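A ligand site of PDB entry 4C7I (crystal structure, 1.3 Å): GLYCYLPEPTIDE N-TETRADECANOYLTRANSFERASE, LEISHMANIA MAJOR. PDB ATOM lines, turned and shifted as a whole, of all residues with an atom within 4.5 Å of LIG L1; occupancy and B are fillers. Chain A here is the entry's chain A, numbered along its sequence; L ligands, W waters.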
ATOM      1  N   TYR A  70      -7.164   1.197 -26.442  1.00  0.00           N
ATOM      2  CA  TYR A  70      -7.655  -0.236 -26.360  1.00  0.00           C
ATOM      3  C   TYR A  70      -6.616  -1.108 -25.661  1.00  0.00           C
ATOM      4  O   TYR A  70      -5.724  -0.665 -24.923  1.00  0.00           O
ATOM      5  CB  TYR A  70      -8.101  -0.696 -27.686  1.00  0.00           C
ATOM      6  CG  TYR A  70      -9.076  -1.907 -27.689  1.00  0.00           C
ATOM      7  CD1 TYR A  70     -10.171  -1.997 -26.851  1.00  0.00           C
ATOM      8  CD2 TYR A  70      -8.760  -2.985 -28.602  1.00  0.00           C
ATOM      9  CE1 TYR A  70     -11.006  -3.111 -26.903  1.00  0.00           C
ATOM     10  CE2 TYR A  70      -9.606  -4.139 -28.638  1.00  0.00           C
ATOM     11  CZ  TYR A  70     -10.704  -4.135 -27.803  1.00  0.00           C
ATOM     12  OH  TYR A  70     -11.587  -5.260 -27.807  1.00  0.00           O
ATOM     13  N   VAL A  71      -6.761  -2.445 -25.807  1.00  0.00           N
ATOM     14  CA  VAL A  71      -6.022  -3.414 -24.948  1.00  0.00           C
ATOM     15  C   VAL A  71      -4.510  -3.374 -25.261  1.00  0.00           C
ATOM     16  O   VAL A  71      -4.064  -3.379 -26.379  1.00  0.00           O
ATOM     17  CB  VAL A  71      -6.550  -4.867 -25.232  1.00  0.00           C
ATOM     18  CG1 VAL A  71      -5.860  -5.869 -24.374  1.00  0.00           C
ATOM     19  CG2 VAL A  71      -8.092  -5.000 -25.039  1.00  0.00           C
ATOM     20  N   GLU A  72      -3.793  -3.429 -24.131  1.00  0.00           N
ATOM     21  CA  GLU A  72      -2.343  -3.597 -24.089  1.00  0.00           C
ATOM     22  C   GLU A  72      -1.947  -4.923 -23.534  1.00  0.00           C
ATOM     23  O   GLU A  72      -2.750  -5.546 -22.828  1.00  0.00           O
ATOM     24  CB  GLU A  72      -1.698  -2.479 -23.246  1.00  0.00           C
ATOM     25  CG  GLU A  72      -2.117  -1.113 -23.756  1.00  0.00           C
ATOM     26  CD  GLU A  72      -1.620   0.080 -22.956  1.00  0.00           C
ATOM     27  OE1 GLU A  72      -1.029  -0.107 -21.912  1.00  0.00           O
ATOM     28  OE2 GLU A  72      -1.933   1.228 -23.372  1.00  0.00           O
ATOM     29  N   ASP A  73      -0.721  -5.404 -23.796  1.00  0.00           N
ATOM     30  CA  ASP A  73      -0.242  -6.577 -23.016  1.00  0.00           C
ATOM     31  C   ASP A  73      -0.099  -6.067 -21.525  1.00  0.00           C
ATOM     32  O   ASP A  73      -0.183  -4.876 -21.193  1.00  0.00           O
ATOM     33  CB  ASP A  73       1.088  -7.056 -23.560  1.00  0.00           C
ATOM     34  CG  ASP A  73       2.133  -6.100 -23.263  1.00  0.00           C
ATOM     35  OD1 ASP A  73       2.080  -4.954 -23.792  1.00  0.00           O
ATOM     36  OD2 ASP A  73       3.114  -6.368 -22.462  1.00  0.00           O
ATOM     37  N   ASP A  74       0.235  -7.043 -20.665  1.00  0.00           N
ATOM     38  CA  ASP A  74       0.289  -6.747 -19.217  1.00  0.00           C
ATOM     39  C   ASP A  74       1.392  -5.849 -18.817  1.00  0.00           C
ATOM     40  O   ASP A  74       1.363  -5.208 -17.706  1.00  0.00           O
ATOM     41  CB  ASP A  74       0.314  -8.071 -18.416  1.00  0.00           C
ATOM     42  CG  ASP A  74       1.661  -8.727 -18.422  1.00  0.00           C
ATOM     43  OD1 ASP A  74       2.610  -8.461 -19.231  1.00  0.00           O
ATOM     44  OD2 ASP A  74       1.786  -9.618 -17.590  1.00  0.00           O
ATOM     45  N   ASP A  75       2.388  -5.699 -19.660  1.00  0.00           N
ATOM     46  CA  ASP A  75       3.536  -4.795 -19.386  1.00  0.00           C
ATOM     47  C   ASP A  75       3.455  -3.493 -20.119  1.00  0.00           C
ATOM     48  O   ASP A  75       4.374  -2.688 -20.142  1.00  0.00           O
ATOM     49  CB  ASP A  75       4.886  -5.449 -19.658  1.00  0.00           C
ATOM     50  CG  ASP A  75       5.176  -6.588 -18.716  1.00  0.00           C
ATOM     51  OD1 ASP A  75       5.127  -6.322 -17.521  1.00  0.00           O
ATOM     52  OD2 ASP A  75       5.302  -7.820 -19.069  1.00  0.00           O
ATOM     53  N   MET A  77       3.572  -2.678 -23.282  1.00  0.00           N
ATOM     54  CA  MET A  77       4.538  -2.594 -24.333  1.00  0.00           C
ATOM     55  C   MET A  77       4.011  -2.522 -25.764  1.00  0.00           C
ATOM     56  O   MET A  77       4.646  -2.037 -26.681  1.00  0.00           O
ATOM     57  CB  MET A  77       5.436  -3.842 -24.190  1.00  0.00           C
ATOM     58  CG  MET A  77       6.329  -3.769 -22.919  1.00  0.00           C
ATOM     59  SD  MET A  77       7.268  -5.293 -22.612  1.00  0.00           S
ATOM     60  CE  MET A  77       8.314  -5.313 -24.014  1.00  0.00           C
ATOM     61  N   PHE A  78       2.785  -3.062 -25.924  1.00  0.00           N
ATOM     62  CA  PHE A  78       2.095  -3.215 -27.235  1.00  0.00           C
ATOM     63  C   PHE A  78       0.645  -2.856 -27.001  1.00  0.00           C
ATOM     64  O   PHE A  78       0.081  -3.278 -25.975  1.00  0.00           O
ATOM     65  CB  PHE A  78       2.215  -4.677 -27.735  1.00  0.00           C
ATOM     66  CG  PHE A  78       3.641  -5.211 -27.792  1.00  0.00           C
ATOM     67  CD1 PHE A  78       4.522  -4.758 -28.795  1.00  0.00           C
ATOM     68  CD2 PHE A  78       4.150  -6.005 -26.782  1.00  0.00           C
ATOM     69  CE1 PHE A  78       5.837  -5.210 -28.799  1.00  0.00           C
ATOM     70  CE2 PHE A  78       5.491  -6.379 -26.776  1.00  0.00           C
ATOM     71  CZ  PHE A  78       6.316  -5.961 -27.810  1.00  0.00           C
ATOM     72  N   PHE A  80      -3.119  -2.933 -29.280  1.00  0.00           N
ATOM     73  CA  PHE A  80      -3.728  -3.219 -30.579  1.00  0.00           C
ATOM     74  C   PHE A  80      -3.980  -1.937 -31.409  1.00  0.00           C
ATOM     75  O   PHE A  80      -4.375  -0.892 -30.849  1.00  0.00           O
ATOM     76  CB  PHE A  80      -5.128  -3.907 -30.383  1.00  0.00           C
ATOM     77  CG  PHE A  80      -5.069  -5.290 -29.891  1.00  0.00           C
ATOM     78  CD1 PHE A  80      -4.376  -6.291 -30.537  1.00  0.00           C
ATOM     79  CD2 PHE A  80      -5.762  -5.572 -28.673  1.00  0.00           C
ATOM     80  CE1 PHE A  80      -4.477  -7.628 -30.062  1.00  0.00           C
ATOM     81  CE2 PHE A  80      -5.788  -6.861 -28.144  1.00  0.00           C
ATOM     82  CZ  PHE A  80      -5.179  -7.893 -28.833  1.00  0.00           C
ATOM     83  N   ASN A 157     -17.892  -6.918 -28.587  1.00  0.00           N
ATOM     84  CA  ASN A 157     -16.410  -6.742 -28.799  1.00  0.00           C
ATOM     85  C   ASN A 157     -16.180  -5.242 -28.661  1.00  0.00           C
ATOM     86  O   ASN A 157     -17.055  -4.382 -28.644  1.00  0.00           O
ATOM     87  CB  ASN A 157     -16.053  -7.251 -30.220  1.00  0.00           C
ATOM     88  CG  ASN A 157     -14.591  -7.631 -30.339  1.00  0.00           C
ATOM     89  OD1 ASN A 157     -13.745  -7.440 -29.493  1.00  0.00           O
ATOM     90  ND2 ASN A 157     -14.290  -8.323 -31.531  1.00  0.00           N
ATOM     91  N   THR A 193     -15.676 -12.184 -24.823  1.00  0.00           N
ATOM     92  CA  THR A 193     -14.369 -12.695 -24.394  1.00  0.00           C
ATOM     93  C   THR A 193     -13.631 -11.580 -23.687  1.00  0.00           C
ATOM     94  O   THR A 193     -13.812 -10.379 -24.010  1.00  0.00           O
ATOM     95  CB  THR A 193     -13.503 -13.316 -25.487  1.00  0.00           C
ATOM     96  OG1 THR A 193     -13.339 -12.379 -26.563  1.00  0.00           O
ATOM     97  CG2 THR A 193     -14.122 -14.572 -26.083  1.00  0.00           C
ATOM     98  N   GLY A 195      -9.383 -10.815 -21.784  1.00  0.00           N
ATOM     99  CA  GLY A 195      -8.103 -11.285 -21.250  1.00  0.00           C
ATOM    100  C   GLY A 195      -8.105 -11.347 -19.785  1.00  0.00           C
ATOM    101  O   GLY A 195      -7.227 -12.053 -19.173  1.00  0.00           O
ATOM    102  N   TYR A 207      -2.994 -18.071 -25.068  1.00  0.00           N
ATOM    103  CA  TYR A 207      -2.491 -17.651 -26.362  1.00  0.00           C
ATOM    104  C   TYR A 207      -1.225 -18.344 -26.709  1.00  0.00           C
ATOM    105  O   TYR A 207      -0.370 -18.644 -25.837  1.00  0.00           O
ATOM    106  CB  TYR A 207      -2.172 -16.133 -26.341  1.00  0.00           C
ATOM    107  CG  TYR A 207      -3.414 -15.305 -26.643  1.00  0.00           C
ATOM    108  CD1 TYR A 207      -4.263 -14.849 -25.624  1.00  0.00           C
ATOM    109  CD2 TYR A 207      -3.720 -14.915 -27.998  1.00  0.00           C
ATOM    110  CE1 TYR A 207      -5.400 -14.074 -25.926  1.00  0.00           C
ATOM    111  CE2 TYR A 207      -4.881 -14.126 -28.270  1.00  0.00           C
ATOM    112  CZ  TYR A 207      -5.663 -13.734 -27.230  1.00  0.00           C
ATOM    113  OH  TYR A 207      -6.782 -12.963 -27.494  1.00  0.00           O
ATOM    114  N   HIS A 209       1.987 -18.335 -29.938  1.00  0.00           N
ATOM    115  CA  HIS A 209       2.633 -17.413 -30.862  1.00  0.00           C
ATOM    116  C   HIS A 209       3.660 -18.189 -31.666  1.00  0.00           C
ATOM    117  O   HIS A 209       4.526 -18.942 -31.091  1.00  0.00           O
ATOM    118  CB  HIS A 209       3.371 -16.302 -30.120  1.00  0.00           C
ATOM    119  CG  HIS A 209       2.524 -15.595 -29.118  1.00  0.00           C
ATOM    120  ND1 HIS A 209       1.574 -14.693 -29.558  1.00  0.00           N
ATOM    121  CD2 HIS A 209       2.423 -15.631 -27.786  1.00  0.00           C
ATOM    122  CE1 HIS A 209       0.942 -14.210 -28.479  1.00  0.00           C
ATOM    123  NE2 HIS A 209       1.437 -14.769 -27.382  1.00  0.00           N
ATOM    124  N   ARG A 221      11.276  -6.663 -28.158  1.00  0.00           N
ATOM    125  CA  ARG A 221      10.986  -7.372 -26.916  1.00  0.00           C
ATOM    126  C   ARG A 221       9.574  -7.930 -26.833  1.00  0.00           C
ATOM    127  O   ARG A 221       9.037  -8.143 -25.744  1.00  0.00           O
ATOM    128  CB  ARG A 221      11.341  -6.568 -25.602  1.00  0.00           C
ATOM    129  CG  ARG A 221      12.785  -6.079 -25.486  1.00  0.00           C
ATOM    130  CD  ARG A 221      13.751  -7.095 -25.995  1.00  0.00           C
ATOM    131  NE  ARG A 221      14.534  -6.476 -27.068  1.00  0.00           N
ATOM    132  CZ  ARG A 221      15.788  -6.072 -26.927  1.00  0.00           C
ATOM    133  NH1 ARG A 221      16.401  -6.216 -25.756  1.00  0.00           N
ATOM    134  NH2 ARG A 221      16.378  -5.519 -27.935  1.00  0.00           N
ATOM    135  N   PHE A 222       9.043  -8.343 -27.994  1.00  0.00           N
ATOM    136  CA  PHE A 222       7.886  -9.295 -28.009  1.00  0.00           C
ATOM    137  C   PHE A 222       8.330 -10.644 -27.550  1.00  0.00           C
ATOM    138  O   PHE A 222       7.546 -11.355 -26.874  1.00  0.00           O
ATOM    139  CB  PHE A 222       7.334  -9.351 -29.391  1.00  0.00           C
ATOM    140  CG  PHE A 222       6.057 -10.149 -29.520  1.00  0.00           C
ATOM    141  CD1 PHE A 222       4.810  -9.542 -29.306  1.00  0.00           C
ATOM    142  CD2 PHE A 222       6.151 -11.487 -29.826  1.00  0.00           C
ATOM    143  CE1 PHE A 222       3.622 -10.308 -29.384  1.00  0.00           C
ATOM    144  CE2 PHE A 222       4.931 -12.221 -29.943  1.00  0.00           C
ATOM    145  CZ  PHE A 222       3.750 -11.620 -29.737  1.00  0.00           C
ATOM    146  N   SER A 223       9.562 -11.061 -27.927  1.00  0.00           N
ATOM    147  CA  SER A 223      10.150 -12.352 -27.417  1.00  0.00           C
ATOM    148  C   SER A 223      11.625 -12.148 -27.140  1.00  0.00           C
ATOM    149  O   SER A 223      12.135 -11.088 -27.363  1.00  0.00           O
ATOM    150  CB  SER A 223      10.110 -13.437 -28.478  1.00  0.00           C
ATOM    151  OG  SER A 223       9.067 -13.252 -29.386  1.00  0.00           O
ATOM    152  N   TYR A 243      13.296 -20.828 -37.072  1.00  0.00           N
ATOM    153  CA  TYR A 243      11.939 -20.419 -37.493  1.00  0.00           C
ATOM    154  C   TYR A 243      11.759 -20.223 -38.967  1.00  0.00           C
ATOM    155  O   TYR A 243      10.681 -19.847 -39.455  1.00  0.00           O
ATOM    156  CB  TYR A 243      11.531 -19.109 -36.764  1.00  0.00           C
ATOM    157  CG  TYR A 243      11.241 -19.392 -35.246  1.00  0.00           C
ATOM    158  CD1 TYR A 243      10.161 -20.151 -34.884  1.00  0.00           C
ATOM    159  CD2 TYR A 243      11.963 -18.810 -34.203  1.00  0.00           C
ATOM    160  CE1 TYR A 243       9.757 -20.343 -33.578  1.00  0.00           C
ATOM    161  CE2 TYR A 243      11.616 -18.996 -32.858  1.00  0.00           C
ATOM    162  CZ  TYR A 243      10.494 -19.767 -32.587  1.00  0.00           C
ATOM    163  OH  TYR A 243      10.183 -19.932 -31.253  1.00  0.00           O
ATOM    164  N   GLY A 383       4.681 -21.380 -29.498  1.00  0.00           N
ATOM    165  CA  GLY A 383       4.952 -21.398 -28.005  1.00  0.00           C
ATOM    166  C   GLY A 383       3.917 -20.591 -27.275  1.00  0.00           C
ATOM    167  O   GLY A 383       3.379 -19.583 -27.784  1.00  0.00           O
ATOM    168  N   ALA A 384       3.540 -21.032 -26.059  1.00  0.00           N
ATOM    169  CA  ALA A 384       2.610 -20.271 -25.194  1.00  0.00           C
ATOM    170  C   ALA A 384       3.140 -18.890 -24.878  1.00  0.00           C
ATOM    171  O   ALA A 384       4.298 -18.749 -24.500  1.00  0.00           O
ATOM    172  CB  ALA A 384       2.290 -21.064 -23.936  1.00  0.00           C
ATOM    173  N   GLY A 385       2.235 -17.905 -24.963  1.00  0.00           N
ATOM    174  CA  GLY A 385       2.591 -16.546 -24.477  1.00  0.00           C
ATOM    175  C   GLY A 385       2.187 -16.359 -23.042  1.00  0.00           C
ATOM    176  O   GLY A 385       1.829 -17.298 -22.320  1.00  0.00           O
ATOM    177  N   ASP A 386       2.137 -15.071 -22.685  1.00  0.00           N
ATOM    178  CA  ASP A 386       1.757 -14.689 -21.296  1.00  0.00           C
ATOM    179  C   ASP A 386       0.311 -14.375 -21.096  1.00  0.00           C
ATOM    180  O   ASP A 386      -0.074 -14.077 -19.909  1.00  0.00           O
ATOM    181  CB  ASP A 386       2.714 -13.619 -20.749  1.00  0.00           C
ATOM    182  CG  ASP A 386       2.555 -12.290 -21.418  1.00  0.00           C
ATOM    183  OD1 ASP A 386       1.775 -12.122 -22.413  1.00  0.00           O
ATOM    184  OD2 ASP A 386       3.332 -11.316 -20.976  1.00  0.00           O
ATOM    185  N   GLY A 387      -0.516 -14.399 -22.115  1.00  0.00           N
ATOM    186  CA  GLY A 387      -1.934 -14.021 -21.982  1.00  0.00           C
ATOM    187  C   GLY A 387      -2.858 -15.265 -22.091  1.00  0.00           C
ATOM    188  O   GLY A 387      -2.427 -16.372 -22.478  1.00  0.00           O
ATOM    189  N   HIS A 388      -4.087 -14.999 -21.787  1.00  0.00           N
ATOM    190  CA  HIS A 388      -5.171 -16.021 -21.885  1.00  0.00           C
ATOM    191  C   HIS A 388      -6.342 -15.307 -22.542  1.00  0.00           C
ATOM    192  O   HIS A 388      -6.512 -14.039 -22.512  1.00  0.00           O
ATOM    193  CB  HIS A 388      -5.620 -16.501 -20.496  1.00  0.00           C
ATOM    194  CG  HIS A 388      -4.556 -17.273 -19.759  1.00  0.00           C
ATOM    195  ND1 HIS A 388      -3.586 -16.668 -18.979  1.00  0.00           N
ATOM    196  CD2 HIS A 388      -4.388 -18.599 -19.599  1.00  0.00           C
ATOM    197  CE1 HIS A 388      -2.848 -17.598 -18.383  1.00  0.00           C
ATOM    198  NE2 HIS A 388      -3.316 -18.773 -18.766  1.00  0.00           N
ATOM    199  N   LEU A 389      -7.236 -16.088 -23.147  1.00  0.00           N
ATOM    200  CA  LEU A 389      -8.554 -15.563 -23.552  1.00  0.00           C
ATOM    201  C   LEU A 389      -9.592 -16.398 -22.798  1.00  0.00           C
ATOM    202  O   LEU A 389      -9.547 -17.640 -22.765  1.00  0.00           O
ATOM    203  CB  LEU A 389      -8.804 -15.673 -25.063  1.00  0.00           C
ATOM    204  CG  LEU A 389     -10.015 -14.882 -25.564  1.00  0.00           C
ATOM    205  CD1 LEU A 389      -9.762 -13.348 -25.332  1.00  0.00           C
ATOM    206  CD2 LEU A 389     -10.264 -15.153 -27.017  1.00  0.00           C
ATOM    207  N   MET A 410     -12.825 -15.251 -31.989  1.00  0.00           N
ATOM    208  CA  MET A 410     -13.238 -13.822 -31.798  1.00  0.00           C
ATOM    209  C   MET A 410     -12.114 -12.874 -32.397  1.00  0.00           C
ATOM    210  O   MET A 410     -10.861 -13.066 -32.322  1.00  0.00           O
ATOM    211  CB  MET A 410     -13.744 -13.472 -30.339  1.00  0.00           C
ATOM    212  CG  MET A 410     -15.185 -13.925 -29.859  1.00  0.00           C
ATOM    213  SD  MET A 410     -15.996 -12.708 -28.737  1.00  0.00           S
ATOM    214  CE  MET A 410     -16.975 -13.993 -28.006  1.00  0.00           C
HETATM  215  O1  LIG L   1       0.856 -10.809 -26.959  1.00  0.00           O
HETATM  216  C1  LIG L   1       0.912 -11.290 -25.812  1.00  0.00           C
HETATM  217  N1  LIG L   1       2.089 -11.611 -25.272  1.00  0.00           N
HETATM  218  C2  LIG L   1       3.312 -11.643 -25.964  1.00  0.00           C
HETATM  219  C3  LIG L   1       4.122 -10.345 -25.655  1.00  0.00           C
HETATM  220  C4  LIG L   1       4.518 -10.260 -24.160  1.00  0.00           C
HETATM  221  C5  LIG L   1       5.230  -8.889 -23.837  1.00  0.00           C
HETATM  222  C6  LIG L   1       5.559  -8.799 -22.335  1.00  0.00           C
HETATM  223  N2  LIG L   1       4.370  -8.809 -21.510  1.00  0.00           N
HETATM  224  C7  LIG L   1       4.093 -12.880 -25.620  1.00  0.00           C
HETATM  225  N3  LIG L   1       5.146 -13.114 -26.400  1.00  0.00           N
HETATM  226  C8  LIG L   1       5.993 -14.248 -26.232  1.00  0.00           C
HETATM  227  C9  LIG L   1       6.290 -14.843 -27.634  1.00  0.00           C
HETATM  228  C10 LIG L   1       7.178 -16.064 -27.552  1.00  0.00           C
HETATM  229  C11 LIG L   1       7.686 -16.486 -28.980  1.00  0.00           C
HETATM  230  C12 LIG L   1       8.608 -17.709 -28.856  1.00  0.00           C
HETATM  231  C13 LIG L   1       7.848 -18.894 -28.259  1.00  0.00           C
HETATM  232  C14 LIG L   1       7.255 -18.480 -26.845  1.00  0.00           C
HETATM  233  C15 LIG L   1       6.380 -17.220 -26.922  1.00  0.00           C
HETATM  234  O2  LIG L   1       3.780 -13.580 -24.667  1.00  0.00           O
HETATM  235  C16 LIG L   1      -0.325 -11.643 -25.023  1.00  0.00           C
HETATM  236  C17 LIG L   1      -0.867 -13.088 -25.440  1.00  0.00           C
HETATM  237  O3  LIG L   1       0.056 -14.023 -25.035  1.00  0.00           O
HETATM  238  N4  LIG L   1      -1.373 -10.640 -25.285  1.00  0.00           N
HETATM  239  C18 LIG L   1      -2.051 -10.066 -24.268  1.00  0.00           C
HETATM  240  O4  LIG L   1      -1.972 -10.539 -23.123  1.00  0.00           O
HETATM  241  C19 LIG L   1      -2.978  -8.949 -24.622  1.00  0.00           C
HETATM  242  C20 LIG L   1      -4.254  -9.522 -25.058  1.00  0.00           C
HETATM  243  C21 LIG L   1      -4.998 -10.505 -24.149  1.00  0.00           C
HETATM  244  C22 LIG L   1      -6.466 -10.598 -24.668  1.00  0.00           C
HETATM  245  C23 LIG L   1      -7.505  -9.471 -24.879  1.00  0.00           C
HETATM  246  C24 LIG L   1      -8.703  -9.797 -25.724  1.00  0.00           C
HETATM  247  C25 LIG L   1      -9.802  -8.699 -25.840  1.00  0.00           C
HETATM  248  C26 LIG L   1     -10.954  -9.403 -26.458  1.00  0.00           C
HETATM  249  C27 LIG L   1     -12.225  -8.620 -26.732  1.00  0.00           C
HETATM  250  O5  LIG L   1     -13.228  -9.542 -27.266  1.00  0.00           O
HETATM  251  S1  LG2 L   2     -12.721  -7.178 -23.361  1.00  0.00           S
HETATM  252  C1  LG2 L   2     -11.640  -5.789 -23.783  1.00  0.00           C
HETATM  253  C2  LG2 L   2     -11.998  -4.600 -22.859  1.00  0.00           C
HETATM  254  N1  LG2 L   2     -11.214  -3.416 -23.215  1.00  0.00           N
HETATM  255  C3  LG2 L   2     -10.053  -3.109 -22.738  1.00  0.00           C
HETATM  256  O1  LG2 L   2      -9.482  -3.834 -21.892  1.00  0.00           O
HETATM  257  C4  LG2 L   2      -9.413  -1.822 -23.204  1.00  0.00           C
HETATM  258  C5  LG2 L   2      -8.643  -1.084 -22.081  1.00  0.00           C
HETATM  259  N2  LG2 L   2      -9.479  -0.836 -20.881  1.00  0.00           N
HETATM  260  C6  LG2 L   2     -10.612  -0.138 -20.841  1.00  0.00           C
HETATM  261  O2  LG2 L   2     -10.964   0.502 -21.858  1.00  0.00           O
HETATM  262  C7  LG2 L   2     -11.287   0.032 -19.500  1.00  0.00           C
HETATM  263  O3  LG2 L   2     -10.333  -0.400 -18.512  1.00  0.00           O
HETATM  264  C8  LG2 L   2     -12.545  -0.847 -19.442  1.00  0.00           C
HETATM  265  C9  LG2 L   2     -13.187  -0.869 -18.084  1.00  0.00           C
HETATM  266  C10 LG2 L   2     -12.261  -2.371 -19.796  1.00  0.00           C
HETATM  267  C11 LG2 L   2     -13.604  -0.371 -20.462  1.00  0.00           C
HETATM  268  N3  LG2 L   2     -15.417  -6.496 -19.436  1.00  0.00           N
HETATM  269  O4  LG2 L   2     -14.897   2.091 -13.429  1.00  0.00           O
HETATM  270  P1  LG2 L   2     -15.154   1.352 -14.742  1.00  0.00           P
HETATM  271  C12 LG2 L   2     -15.748  -4.133 -14.877  1.00  0.00           C
HETATM  272  C13 LG2 L   2     -16.440  -6.320 -18.549  1.00  0.00           C
HETATM  273  O5  LG2 L   2     -15.712   2.097 -15.817  1.00  0.00           O
HETATM  274  P2  LG2 L   2     -12.718   1.131 -16.349  1.00  0.00           P
HETATM  275  C14 LG2 L   2     -14.181  -6.769 -24.227  1.00  0.00           C
HETATM  276  O6  LG2 L   2     -14.211  -5.900 -25.053  1.00  0.00           O
HETATM  277  C15 LG2 L   2     -15.076  -4.238 -13.516  1.00  0.00           C
HETATM  278  O7  LG2 L   2     -15.025  -5.555 -13.051  1.00  0.00           O
HETATM  279  N4  LG2 L   2     -16.412  -5.717 -17.374  1.00  0.00           N
HETATM  280  O8  LG2 L   2     -13.700   0.697 -15.177  1.00  0.00           O
HETATM  281  C16 LG2 L   2     -15.436  -7.579 -23.881  1.00  0.00           C
HETATM  282  C17 LG2 L   2     -15.993  -3.286 -12.737  1.00  0.00           C
HETATM  283  O9  LG2 L   2     -17.185  -3.963 -12.345  1.00  0.00           O
HETATM  284  P3  LG2 L   2     -17.345  -4.580 -10.814  1.00  0.00           P
HETATM  285  C18 LG2 L   2     -15.203  -5.256 -17.069  1.00  0.00           C
HETATM  286  O10 LG2 L   2     -12.744   2.561 -16.504  1.00  0.00           O
HETATM  287  C19 LG2 L   2     -16.357  -6.629 -23.110  1.00  0.00           C
HETATM  288  C20 LG2 L   2     -16.363  -2.206 -13.691  1.00  0.00           C
HETATM  289  O11 LG2 L   2     -16.010  -2.753 -15.065  1.00  0.00           O
HETATM  290  C21 LG2 L   2     -14.100  -5.356 -17.878  1.00  0.00           C
HETATM  291  O12 LG2 L   2     -11.438   0.424 -16.067  1.00  0.00           O
HETATM  292  C22 LG2 L   2     -17.539  -7.410 -22.509  1.00  0.00           C
HETATM  293  C23 LG2 L   2     -15.572  -0.937 -13.571  1.00  0.00           C
HETATM  294  O13 LG2 L   2     -15.954   0.056 -14.470  1.00  0.00           O
HETATM  295  C24 LG2 L   2     -14.234  -6.050 -19.101  1.00  0.00           C
HETATM  296  N5  LG2 L   2     -13.216  -6.260 -19.975  1.00  0.00           N
HETATM  297  O14 LG2 L   2     -13.383   0.555 -17.709  1.00  0.00           O
HETATM  298  C25 LG2 L   2     -18.476  -6.428 -21.694  1.00  0.00           C
HETATM  299  N6  LG2 L   2     -13.008  -4.747 -17.272  1.00  0.00           N
HETATM  300  O15 LG2 L   2     -17.209  -3.324  -9.929  1.00  0.00           O
HETATM  301  C26 LG2 L   2     -19.725  -7.159 -21.111  1.00  0.00           C
HETATM  302  C27 LG2 L   2     -13.511  -4.240 -16.102  1.00  0.00           C
HETATM  303  O16 LG2 L   2     -18.674  -5.284 -10.716  1.00  0.00           O
HETATM  304  C28 LG2 L   2     -20.792  -7.471 -22.148  1.00  0.00           C
HETATM  305  N7  LG2 L   2     -14.818  -4.541 -15.983  1.00  0.00           N
HETATM  306  O17 LG2 L   2     -16.158  -5.538 -10.631  1.00  0.00           O
HETATM  307  C29 LG2 L   2     -22.071  -8.062 -21.499  1.00  0.00           C
HETATM  308  C30 LG2 L   2     -23.193  -8.370 -22.453  1.00  0.00           C
HETATM  309  C31 LG2 L   2     -23.870  -7.095 -22.950  1.00  0.00           C
HETATM  310  C32 LG2 L   2     -25.024  -7.327 -23.969  1.00  0.00           C
HETATM  311  C33 LG2 L   2     -26.108  -8.242 -23.422  1.00  0.00           C
HETATM  312  C34 LG2 L   2     -27.231  -8.455 -24.461  1.00  0.00           C
HETATM  313  C35 LG2 L   2     -28.235  -9.527 -24.021  1.00  0.00           C
HETATM  314  O   HOH W   1       0.364  -9.793 -21.595  1.00  0.00           O
HETATM  315  O   HOH W   2      -0.562 -11.342 -29.323  1.00  0.00           O
HETATM  316  O   HOH W   3     -15.741  -9.791 -26.469  1.00  0.00           O
HETATM  317  O   HOH W   4       5.572 -14.527 -22.759  1.00  0.00           O
HETATM  318  O   HOH W   5      -3.535 -10.037 -20.915  1.00  0.00           O
HETATM  319  O   HOH W   6       7.305 -18.872 -31.790  1.00  0.00           O
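OD2 of Asp 73 sits at hydrogen-bond distance from N of Asp 75 (3.0 Å).
O of Gly 383 sits at hydrogen-bond distance from N of His 209.
The backbone NH (N) of Phe 78 sits at hydrogen-bond distance from the side-chain carboxylate (OD1) of Asp 73 (2.9 Å).
The backbone NH (N) of Met 77 lies within hydrogen-bond range of the side-chain carboxylate (OD1) of Asp 73.
The side-chain hydroxyl (OG1) of Thr 193 lies within hydrogen-bond range of the side-chain sulfur (SD) of Met 410, 3.4 Å away.
The backbone carbonyl oxygen of Gly 387 sits at hydrogen-bond distance from the backbone NH of Tyr 207, 3.1 Å away.
The backbone carbonyl oxygen of Tyr 207 lies within hydrogen-bond range of the backbone NH of Gly 385.
O of Val 71 lies within hydrogen-bond range of N of Phe 80 (3.1 Å).
An oxygen (O2) of LIG L1 lies within hydrogen-bond range of the backbone NH (N) of Asp 386 (3.0 Å).
The side-chain carboxylate (OD2) of Asp 386 is in salt-bridge range of a nitrogen (N2) of LIG L1.
OD2 of Asp 75 lies within salt-bridge range of N2 of LIG L1 (2.8 Å).
NE2 of His 209 is in hydrogen-bond range of O3 of LIG L1 (2.8 Å).
N2 of LIG L1 is in salt-bridge range of OD1 of Asp 74, 2.9 Å away.
The side-chain carboxylate (OD2) of Asp 73 lies within salt-bridge range of a nitrogen (N2) of LIG L1 (2.9 Å).
An oxygen (O5) of LIG L1 is in hydrogen-bond range of the backbone carbonyl oxygen (O) of Thr 193 (3.4 Å).
The side-chain hydroxyl (OG1) of Thr 193 sits at hydrogen-bond distance from an oxygen (O5) of LIG L1 (2.9 Å).
An oxygen (O3) of LIG L1 is in hydrogen-bond range of the backbone NH (N) of Gly 387, 3.0 Å away.
The backbone carbonyl oxygen of Phe 222 lies within hydrogen-bond range of a nitrogen (N3) of LIG L1, 3.0 Å away.
The side-chain amide oxygen (OD1) of Asn 157 lies within hydrogen-bond range of an oxygen (O5) of LIG L1.
OH of Tyr 70 touches C27 of LIG L1, at 3.6 Å.
Val 71 touches LIG L1 (CG1 to C23, 3.99 Å).
Glu 72 touches LIG L1 (O to C19, 3.9 Å).
Met 77 touches LIG L1 (SD to C6, 3.9 Å).
Phe 78 touches LIG L1 (CE2 to C5, 3.9 Å).
CA of Gly 195 touches C22 of LIG L1 (3.9 Å).
Tyr 207 touches LIG L1.
Ser 223 touches LIG L1 (OG to C11, 3.5 Å).
Tyr 243 touches LIG L1 (OH to C12, 3.6 Å).
Gly 383 touches LIG L1.
O of Ala 384 touches C15 of LIG L1, at 3.5 Å.
Gly 385 touches LIG L1 (CA to O2, 3.2 Å).
CD1 of Leu 389 touches C24 of LIG L1 (3.7 Å).
The nearest printed residue that does not touch LIG L1 is His 388 (4.1 Å).
Water W3 lies within hydrogen-bond range of an oxygen (O5) of LIG L1 (2.6 Å), the backbone NH of Thr 193 (2.9 Å) and the side-chain sulfur of Met 410 (3.7 Å).
Water W4 lies within hydrogen-bond range of an oxygen (O2) of LIG L1 and the backbone NH of Asp 386.
Water W1 lies within hydrogen-bond range of the side-chain carboxylate of Asp 386, an oxygen (O4) of LIG L1 and the backbone NH of Asp 74.
Water W6 bridges the backbone carbonyl oxygen of His 209 (2.9 Å) and the side-chain hydroxyl of Tyr 243 (3.1 Å).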
